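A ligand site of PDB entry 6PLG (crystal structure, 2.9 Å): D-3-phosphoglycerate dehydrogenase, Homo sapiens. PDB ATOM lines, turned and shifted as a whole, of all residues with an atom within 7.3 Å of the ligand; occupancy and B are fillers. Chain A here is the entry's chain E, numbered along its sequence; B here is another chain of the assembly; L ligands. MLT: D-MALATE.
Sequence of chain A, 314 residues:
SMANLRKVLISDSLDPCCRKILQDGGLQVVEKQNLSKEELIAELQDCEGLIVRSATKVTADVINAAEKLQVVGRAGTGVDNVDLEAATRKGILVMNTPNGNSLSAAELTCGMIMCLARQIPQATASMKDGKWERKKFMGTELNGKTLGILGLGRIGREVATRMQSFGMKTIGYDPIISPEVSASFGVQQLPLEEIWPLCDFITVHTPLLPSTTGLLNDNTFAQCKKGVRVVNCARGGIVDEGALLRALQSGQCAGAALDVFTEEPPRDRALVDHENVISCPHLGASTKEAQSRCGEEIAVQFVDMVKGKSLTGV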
ATOM      1  N   SER A  13      -4.303  38.760 -20.212  1.00  0.00           N
ATOM      2  CA  SER A  13      -2.917  38.225 -20.236  1.00  0.00           C
ATOM      3  C   SER A  13      -3.004  36.707 -20.464  1.00  0.00           C
ATOM      4  O   SER A  13      -3.352  35.967 -19.519  1.00  0.00           O
ATOM      5  CB  SER A  13      -2.156  38.571 -18.973  1.00  0.00           C
ATOM      6  OG  SER A  13      -0.776  38.279 -19.108  1.00  0.00           O
ATOM      7  N   LEU A  14      -2.768  36.282 -21.711  1.00  0.00           N
ATOM      8  CA  LEU A  14      -2.723  34.864 -22.135  1.00  0.00           C
ATOM      9  C   LEU A  14      -1.371  34.628 -22.824  1.00  0.00           C
ATOM     10  O   LEU A  14      -0.872  35.570 -23.494  1.00  0.00           O
ATOM     11  CB  LEU A  14      -3.885  34.629 -23.096  1.00  0.00           C
ATOM     12  CG  LEU A  14      -4.780  33.411 -22.820  1.00  0.00           C
ATOM     13  CD1 LEU A  14      -5.967  33.454 -23.767  1.00  0.00           C
ATOM     14  CD2 LEU A  14      -4.046  32.074 -22.947  1.00  0.00           C
ATOM     15  N   VAL A  52     -10.950  34.481 -23.199  1.00  0.00           N
ATOM     16  CA  VAL A  52     -10.798  35.140 -21.876  1.00  0.00           C
ATOM     17  C   VAL A  52     -10.083  34.187 -20.913  1.00  0.00           C
ATOM     18  O   VAL A  52     -10.111  32.939 -21.165  1.00  0.00           O
ATOM     19  CB  VAL A  52     -12.147  35.596 -21.292  1.00  0.00           C
ATOM     20  CG1 VAL A  52     -12.681  36.839 -21.992  1.00  0.00           C
ATOM     21  CG2 VAL A  52     -13.191  34.487 -21.317  1.00  0.00           C
ATOM     22  N   ARG A  53      -9.471  34.776 -19.885  1.00  0.00           N
ATOM     23  CA  ARG A  53      -8.891  34.041 -18.730  1.00  0.00           C
ATOM     24  C   ARG A  53      -9.880  34.160 -17.577  1.00  0.00           C
ATOM     25  O   ARG A  53     -11.101  33.969 -17.875  1.00  0.00           O
ATOM     26  CB  ARG A  53      -7.489  34.579 -18.417  1.00  0.00           C
ATOM     27  CG  ARG A  53      -6.516  33.542 -17.855  1.00  0.00           C
ATOM     28  CD  ARG A  53      -5.937  33.753 -16.454  1.00  0.00           C
ATOM     29  NE  ARG A  53      -4.496  33.561 -16.292  1.00  0.00           N
ATOM     30  CZ  ARG A  53      -3.620  34.534 -16.070  1.00  0.00           C
ATOM     31  NH1 ARG A  53      -2.341  34.241 -15.883  1.00  0.00           N
ATOM     32  NH2 ARG A  53      -3.995  35.799 -16.052  1.00  0.00           N
ATOM     33  N   SER A  54      -9.450  34.492 -16.350  1.00  0.00           N
ATOM     34  CA  SER A  54     -10.348  34.634 -15.171  1.00  0.00           C
ATOM     35  C   SER A  54     -10.704  36.117 -14.920  1.00  0.00           C
ATOM     36  O   SER A  54     -11.711  36.357 -14.219  1.00  0.00           O
ATOM     37  CB  SER A  54      -9.774  33.971 -13.949  1.00  0.00           C
ATOM     38  OG  SER A  54     -10.279  32.660 -13.812  1.00  0.00           O
ATOM     39  N   ALA A  55      -9.929  37.046 -15.463  1.00  0.00           N
ATOM     40  CA  ALA A  55     -10.060  38.504 -15.211  1.00  0.00           C
ATOM     41  C   ALA A  55     -11.380  39.020 -15.827  1.00  0.00           C
ATOM     42  O   ALA A  55     -12.261  39.406 -15.063  1.00  0.00           O
ATOM     43  CB  ALA A  55      -8.861  39.241 -15.743  1.00  0.00           C
ATOM     44  N   ARG A  74     -12.695  30.027 -23.241  1.00  0.00           N
ATOM     45  CA  ARG A  74     -12.047  30.302 -21.935  1.00  0.00           C
ATOM     46  C   ARG A  74     -10.808  29.402 -21.819  1.00  0.00           C
ATOM     47  O   ARG A  74     -10.955  28.154 -21.871  1.00  0.00           O
ATOM     48  CB  ARG A  74     -13.078  30.098 -20.833  1.00  0.00           C
ATOM     49  CG  ARG A  74     -12.480  29.683 -19.508  1.00  0.00           C
ATOM     50  CD  ARG A  74     -11.438  30.710 -19.135  1.00  0.00           C
ATOM     51  NE  ARG A  74     -11.063  30.965 -17.745  1.00  0.00           N
ATOM     52  CZ  ARG A  74     -11.261  30.177 -16.705  1.00  0.00           C
ATOM     53  NH1 ARG A  74     -11.802  28.993 -16.839  1.00  0.00           N
ATOM     54  NH2 ARG A  74     -10.907  30.629 -15.514  1.00  0.00           N
ATOM     55  N   ALA A  75      -9.626  30.020 -21.737  1.00  0.00           N
ATOM     56  CA  ALA A  75      -8.332  29.334 -21.541  1.00  0.00           C
ATOM     57  C   ALA A  75      -8.167  29.045 -20.051  1.00  0.00           C
ATOM     58  O   ALA A  75      -7.459  29.826 -19.383  1.00  0.00           O
ATOM     59  CB  ALA A  75      -7.227  30.204 -22.102  1.00  0.00           C
ATOM     60  N   GLY A  76      -8.856  28.024 -19.532  1.00  0.00           N
ATOM     61  CA  GLY A  76      -8.751  27.583 -18.130  1.00  0.00           C
ATOM     62  C   GLY A  76      -9.660  26.408 -17.852  1.00  0.00           C
ATOM     63  O   GLY A  76     -10.087  25.754 -18.847  1.00  0.00           O
ATOM     64  N   THR A  77      -9.927  26.116 -16.573  1.00  0.00           N
ATOM     65  CA  THR A  77     -10.848  25.052 -16.138  1.00  0.00           C
ATOM     66  C   THR A  77     -12.143  25.708 -15.653  1.00  0.00           C
ATOM     67  O   THR A  77     -12.049  26.588 -14.786  1.00  0.00           O
ATOM     68  CB  THR A  77     -10.220  24.166 -15.051  1.00  0.00           C
ATOM     69  OG1 THR A  77     -10.371  24.831 -13.787  1.00  0.00           O
ATOM     70  CG2 THR A  77      -8.753  23.867 -15.298  1.00  0.00           C
ATOM     71  N   GLY A  78     -13.283  25.318 -16.212  1.00  0.00           N
ATOM     72  CA  GLY A  78     -14.599  25.903 -15.913  1.00  0.00           C
ATOM     73  C   GLY A  78     -14.886  27.163 -16.713  1.00  0.00           C
ATOM     74  O   GLY A  78     -13.981  27.616 -17.422  1.00  0.00           O
ATOM     75  N   VAL A  79     -16.058  27.749 -16.506  1.00  0.00           N
ATOM     76  CA  VAL A  79     -16.540  28.983 -17.197  1.00  0.00           C
ATOM     77  C   VAL A  79     -17.272  29.872 -16.196  1.00  0.00           C
ATOM     78  O   VAL A  79     -18.244  30.537 -16.598  1.00  0.00           O
ATOM     79  CB  VAL A  79     -17.426  28.597 -18.400  1.00  0.00           C
ATOM     80  CG1 VAL A  79     -16.639  27.930 -19.506  1.00  0.00           C
ATOM     81  CG2 VAL A  79     -18.596  27.691 -18.008  1.00  0.00           C
ATOM     82  N   THR A  97     -11.077  24.288 -21.833  1.00  0.00           N
ATOM     83  CA  THR A  97      -9.744  23.651 -21.938  1.00  0.00           C
ATOM     84  C   THR A  97      -9.624  22.617 -20.824  1.00  0.00           C
ATOM     85  O   THR A  97      -8.934  22.831 -19.839  1.00  0.00           O
ATOM     86  CB  THR A  97      -8.630  24.702 -21.939  1.00  0.00           C
ATOM     87  OG1 THR A  97      -8.921  25.536 -20.833  1.00  0.00           O
ATOM     88  CG2 THR A  97      -8.614  25.596 -23.149  1.00  0.00           C
ATOM     89  N   ASN A 101      -4.517  21.783 -17.666  1.00  0.00           N
ATOM     90  CA  ASN A 101      -4.552  22.554 -16.408  1.00  0.00           C
ATOM     91  C   ASN A 101      -4.542  21.613 -15.191  1.00  0.00           C
ATOM     92  O   ASN A 101      -3.915  21.925 -14.175  1.00  0.00           O
ATOM     93  CB  ASN A 101      -5.766  23.474 -16.339  1.00  0.00           C
ATOM     94  CG  ASN A 101      -5.400  24.842 -15.813  1.00  0.00           C
ATOM     95  OD1 ASN A 101      -4.442  24.964 -15.047  1.00  0.00           O
ATOM     96  ND2 ASN A 101      -6.111  25.856 -16.299  1.00  0.00           N
ATOM     97  N   CYS A 233      -8.572  23.369  -3.346  1.00  0.00           N
ATOM     98  CA  CYS A 233      -7.870  23.915  -4.536  1.00  0.00           C
ATOM     99  C   CYS A 233      -8.783  23.877  -5.773  1.00  0.00           C
ATOM    100  O   CYS A 233      -8.291  24.120  -6.901  1.00  0.00           O
ATOM    101  CB  CYS A 233      -6.597  23.119  -4.813  1.00  0.00           C
ATOM    102  SG  CYS A 233      -5.199  23.613  -3.781  1.00  0.00           S
ATOM    103  N   ALA A 234     -10.080  23.612  -5.560  1.00  0.00           N
ATOM    104  CA  ALA A 234     -11.081  23.410  -6.643  1.00  0.00           C
ATOM    105  C   ALA A 234     -11.898  24.686  -6.841  1.00  0.00           C
ATOM    106  O   ALA A 234     -11.541  25.488  -7.735  1.00  0.00           O
ATOM    107  CB  ALA A 234     -11.944  22.238  -6.302  1.00  0.00           C
ATOM    108  N   ARG A 235     -12.976  24.863  -6.054  1.00  0.00           N
ATOM    109  CA  ARG A 235     -13.870  26.036  -6.171  1.00  0.00           C
ATOM    110  C   ARG A 235     -14.215  26.548  -4.771  1.00  0.00           C
ATOM    111  O   ARG A 235     -14.329  25.721  -3.839  1.00  0.00           O
ATOM    112  CB  ARG A 235     -15.144  25.697  -6.931  1.00  0.00           C
ATOM    113  CG  ARG A 235     -14.982  24.900  -8.211  1.00  0.00           C
ATOM    114  CD  ARG A 235     -14.514  25.782  -9.341  1.00  0.00           C
ATOM    115  NE  ARG A 235     -14.409  25.005 -10.564  1.00  0.00           N
ATOM    116  CZ  ARG A 235     -13.597  25.294 -11.584  1.00  0.00           C
ATOM    117  NH1 ARG A 235     -13.569  24.494 -12.639  1.00  0.00           N
ATOM    118  NH2 ARG A 235     -12.801  26.357 -11.536  1.00  0.00           N
ATOM    119  N   ASP A 259      -6.865  27.649  -1.949  1.00  0.00           N
ATOM    120  CA  ASP A 259      -6.445  28.349  -3.186  1.00  0.00           C
ATOM    121  C   ASP A 259      -7.639  29.126  -3.759  1.00  0.00           C
ATOM    122  O   ASP A 259      -7.432  29.937  -4.682  1.00  0.00           O
ATOM    123  CB  ASP A 259      -5.864  27.375  -4.212  1.00  0.00           C
ATOM    124  CG  ASP A 259      -5.180  28.049  -5.415  1.00  0.00           C
ATOM    125  OD1 ASP A 259      -4.313  28.920  -5.179  1.00  0.00           O
ATOM    126  OD2 ASP A 259      -5.488  27.701  -6.597  1.00  0.00           O
ATOM    127  N   VAL A 260      -8.848  28.903  -3.235  1.00  0.00           N
ATOM    128  CA  VAL A 260     -10.118  29.412  -3.852  1.00  0.00           C
ATOM    129  C   VAL A 260     -11.076  29.927  -2.779  1.00  0.00           C
ATOM    130  O   VAL A 260     -11.167  29.307  -1.679  1.00  0.00           O
ATOM    131  CB  VAL A 260     -10.768  28.315  -4.725  1.00  0.00           C
ATOM    132  CG1 VAL A 260     -10.121  28.285  -6.111  1.00  0.00           C
ATOM    133  CG2 VAL A 260     -10.744  26.944  -4.066  1.00  0.00           C
ATOM    134  N   GLU A 264     -13.615  36.459  -4.886  1.00  0.00           N
ATOM    135  CA  GLU A 264     -12.229  36.450  -5.417  1.00  0.00           C
ATOM    136  C   GLU A 264     -11.936  37.791  -6.075  1.00  0.00           C
ATOM    137  O   GLU A 264     -12.374  38.027  -7.196  1.00  0.00           O
ATOM    138  CB  GLU A 264     -12.067  35.304  -6.417  1.00  0.00           C
ATOM    139  CG  GLU A 264     -11.828  33.967  -5.735  1.00  0.00           C
ATOM    140  CD  GLU A 264     -11.265  32.847  -6.587  1.00  0.00           C
ATOM    141  OE1 GLU A 264     -11.494  31.652  -6.217  1.00  0.00           O
ATOM    142  OE2 GLU A 264     -10.539  33.188  -7.517  1.00  0.00           O
ATOM    143  N   HIS A 282      -5.187  32.087  -5.789  1.00  0.00           N
ATOM    144  CA  HIS A 282      -5.708  31.275  -6.927  1.00  0.00           C
ATOM    145  C   HIS A 282      -4.592  30.992  -7.939  1.00  0.00           C
ATOM    146  O   HIS A 282      -4.633  31.573  -9.050  1.00  0.00           O
ATOM    147  CB  HIS A 282      -6.966  31.961  -7.504  1.00  0.00           C
ATOM    148  CG  HIS A 282      -7.763  31.077  -8.411  1.00  0.00           C
ATOM    149  ND1 HIS A 282      -8.659  31.582  -9.335  1.00  0.00           N
ATOM    150  CD2 HIS A 282      -7.709  29.749  -8.623  1.00  0.00           C
ATOM    151  CE1 HIS A 282      -9.147  30.579 -10.049  1.00  0.00           C
ATOM    152  NE2 HIS A 282      -8.608  29.445  -9.611  1.00  0.00           N
ATOM    153  N   LEU A 283      -3.632  30.118  -7.563  1.00  0.00           N
ATOM    154  CA  LEU A 283      -2.395  29.790  -8.339  1.00  0.00           C
ATOM    155  C   LEU A 283      -2.483  28.379  -8.941  1.00  0.00           C
ATOM    156  O   LEU A 283      -1.440  27.899  -9.444  1.00  0.00           O
ATOM    157  CB  LEU A 283      -1.176  29.879  -7.416  1.00  0.00           C
ATOM    158  CG  LEU A 283      -0.965  31.199  -6.680  1.00  0.00           C
ATOM    159  CD1 LEU A 283       0.068  31.067  -5.592  1.00  0.00           C
ATOM    160  CD2 LEU A 283      -0.545  32.288  -7.638  1.00  0.00           C
ATOM    161  N   GLY A 284      -3.634  27.712  -8.862  1.00  0.00           N
ATOM    162  CA  GLY A 284      -3.820  26.344  -9.374  1.00  0.00           C
ATOM    163  C   GLY A 284      -3.434  26.204 -10.840  1.00  0.00           C
ATOM    164  O   GLY A 284      -2.954  25.108 -11.213  1.00  0.00           O
ATOM    165  N   ALA A 285      -3.634  27.256 -11.644  1.00  0.00           N
ATOM    166  CA  ALA A 285      -3.280  27.301 -13.080  1.00  0.00           C
ATOM    167  C   ALA A 285      -2.175  28.329 -13.332  1.00  0.00           C
ATOM    168  O   ALA A 285      -2.036  28.738 -14.511  1.00  0.00           O
ATOM    169  CB  ALA A 285      -4.516  27.646 -13.869  1.00  0.00           C
ATOM    170  N   SER A 286      -1.477  28.774 -12.255  1.00  0.00           N
ATOM    171  CA  SER A 286      -0.411  29.811 -12.321  1.00  0.00           C
ATOM    172  C   SER A 286       0.962  29.175 -12.611  1.00  0.00           C
ATOM    173  O   SER A 286       1.781  29.099 -11.675  1.00  0.00           O
ATOM    174  CB  SER A 286      -0.408  30.669 -11.076  1.00  0.00           C
ATOM    175  OG  SER A 286      -1.378  31.721 -11.189  1.00  0.00           O
ATOM    176  N   THR A 287       1.142  28.674 -13.840  1.00  0.00           N
ATOM    177  CA  THR A 287       2.359  28.035 -14.356  1.00  0.00           C
ATOM    178  C   THR A 287       2.446  28.258 -15.881  1.00  0.00           C
ATOM    179  O   THR A 287       1.421  27.957 -16.613  1.00  0.00           O
ATOM    180  CB  THR A 287       2.412  26.521 -14.073  1.00  0.00           C
ATOM    181  OG1 THR A 287       1.512  25.854 -14.960  1.00  0.00           O
ATOM    182  CG2 THR A 287       2.090  26.164 -12.638  1.00  0.00           C
ATOM    183  N   GLN A 291      -0.720  27.337 -18.820  1.00  0.00           N
ATOM    184  CA  GLN A 291      -1.406  28.399 -19.583  1.00  0.00           C
ATOM    185  C   GLN A 291      -1.071  28.302 -21.072  1.00  0.00           C
ATOM    186  O   GLN A 291      -1.899  28.739 -21.888  1.00  0.00           O
ATOM    187  CB  GLN A 291      -1.074  29.779 -19.027  1.00  0.00           C
ATOM    188  CG  GLN A 291      -2.275  30.709 -19.177  1.00  0.00           C
ATOM    189  CD  GLN A 291      -3.382  30.371 -18.197  1.00  0.00           C
ATOM    190  OE1 GLN A 291      -3.716  31.128 -17.283  1.00  0.00           O
ATOM    191  NE2 GLN A 291      -3.947  29.172 -18.339  1.00  0.00           N
ATOM    192  N   CYS A 294      -3.300  25.207 -22.237  1.00  0.00           N
ATOM    193  CA  CYS A 294      -4.653  25.815 -22.331  1.00  0.00           C
ATOM    194  C   CYS A 294      -4.710  26.686 -23.582  1.00  0.00           C
ATOM    195  O   CYS A 294      -5.336  26.247 -24.569  1.00  0.00           O
ATOM    196  CB  CYS A 294      -4.998  26.672 -21.117  1.00  0.00           C
ATOM    197  SG  CYS A 294      -5.762  25.856 -19.694  1.00  0.00           S
ATOM    198  N   ARG B 134      -1.990  37.219  -8.274  1.00  0.00           N
ATOM    199  CA  ARG B 134      -1.971  35.952  -9.069  1.00  0.00           C
ATOM    200  C   ARG B 134      -1.191  36.164 -10.367  1.00  0.00           C
ATOM    201  O   ARG B 134      -0.662  35.176 -10.896  1.00  0.00           O
ATOM    202  CB  ARG B 134      -3.392  35.412  -9.285  1.00  0.00           C
ATOM    203  CG  ARG B 134      -3.988  35.492 -10.692  1.00  0.00           C
ATOM    204  CD  ARG B 134      -5.397  34.932 -10.716  1.00  0.00           C
ATOM    205  NE  ARG B 134      -5.392  33.469 -10.797  1.00  0.00           N
ATOM    206  CZ  ARG B 134      -5.816  32.738 -11.828  1.00  0.00           C
ATOM    207  NH1 ARG B 134      -5.728  31.415 -11.765  1.00  0.00           N
ATOM    208  NH2 ARG B 134      -6.345  33.310 -12.899  1.00  0.00           N
HETATM  209  C1  MLT L   1      -8.987  28.360 -13.466  1.00  0.00           C
HETATM  210  O1  MLT L   1      -9.467  28.511 -12.320  1.00  0.00           O
HETATM  211  O2  MLT L   1      -9.412  27.467 -14.235  1.00  0.00           O
HETATM  212  C2  MLT L   1      -7.835  29.277 -13.851  1.00  0.00           C
HETATM  213  O3  MLT L   1      -8.002  30.579 -13.268  1.00  0.00           O
HETATM  214  C3  MLT L   1      -7.642  29.410 -15.362  1.00  0.00           C
HETATM  215  C4  MLT L   1      -6.527  30.354 -15.745  1.00  0.00           C
HETATM  216  O4  MLT L   1      -5.733  30.806 -14.885  1.00  0.00           O
HETATM  217  O5  MLT L   1      -6.440  30.653 -16.955  1.00  0.00           O
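CA of Gly 76 touches C3 of the ligand, at 3.5 Å.
Asn 101 touches the ligand.
Ala 285 touches the ligand (CB to O4, 3.5 Å).
The nearest printed residue that does not touch the ligand is Arg 235 (4.05 Å).
The backbone NH of Thr 77 lies within hydrogen-bond range of an oxygen (O2) of the ligand.
An oxygen (O2) of the ligand lies close to the backbone carbonyl oxygen of Thr 77, at 2.8 Å.
O2 of the ligand lies within hydrogen-bond range of OG1 of Thr 77, 2.8 Å away.
O of Ala 75 lies close to O5 of the ligand (2.8 Å).
An oxygen (O5) of the ligand sits close to the side-chain amide oxygen (OE1) of Gln 291, 2.8 Å away.
NH1 of Arg 134 of chain B is in salt-bridge range of O4 of the ligand, 3.2 Å away.
O1 of the ligand sits at hydrogen-bond distance from NE2 of His 282.
The guanidinium group (NE) of Arg 53 lies within salt-bridge range of an oxygen (O4) of the ligand (3.3 Å).
The side-chain hydroxyl of Ser 54 sits at hydrogen-bond distance from an oxygen (O3) of the ligand (3.1 Å).
O2 of the ligand lies within salt-bridge range of NH2 of Arg 74 (3.7 Å).
The backbone carbonyl oxygen (O) of Thr 77 lies within hydrogen-bond range of the guanidinium group (NH1) of Arg 74 (3.2 Å).
The backbone carbonyl oxygen of Thr 77 lies within hydrogen-bond range of the guanidinium group of Arg 235 (3.3 Å).
OE1 of Gln 291 lies within hydrogen-bond range of NE of Arg 53 (2.7 Å).
The guanidinium group of Arg 134 of chain B sits at hydrogen-bond distance from the backbone carbonyl oxygen of His 282 (2.7 Å).
The backbone carbonyl oxygen (O) of Arg 53 sits at hydrogen-bond distance from the guanidinium group (NE) of Arg 74, at 3.0 Å.
The guanidinium group (NH1) of Arg 74 sits at hydrogen-bond distance from the backbone carbonyl oxygen (O) of Gly 78 (2.6 Å).
The side-chain hydroxyl (OG1) of Thr 97 is in hydrogen-bond range of the backbone carbonyl oxygen (O) of Arg 74 (3.5 Å).
The side-chain sulfur (SG) of Cys 294 lies within hydrogen-bond range of the backbone NH (N) of Gly 76, 3.8 Å away.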
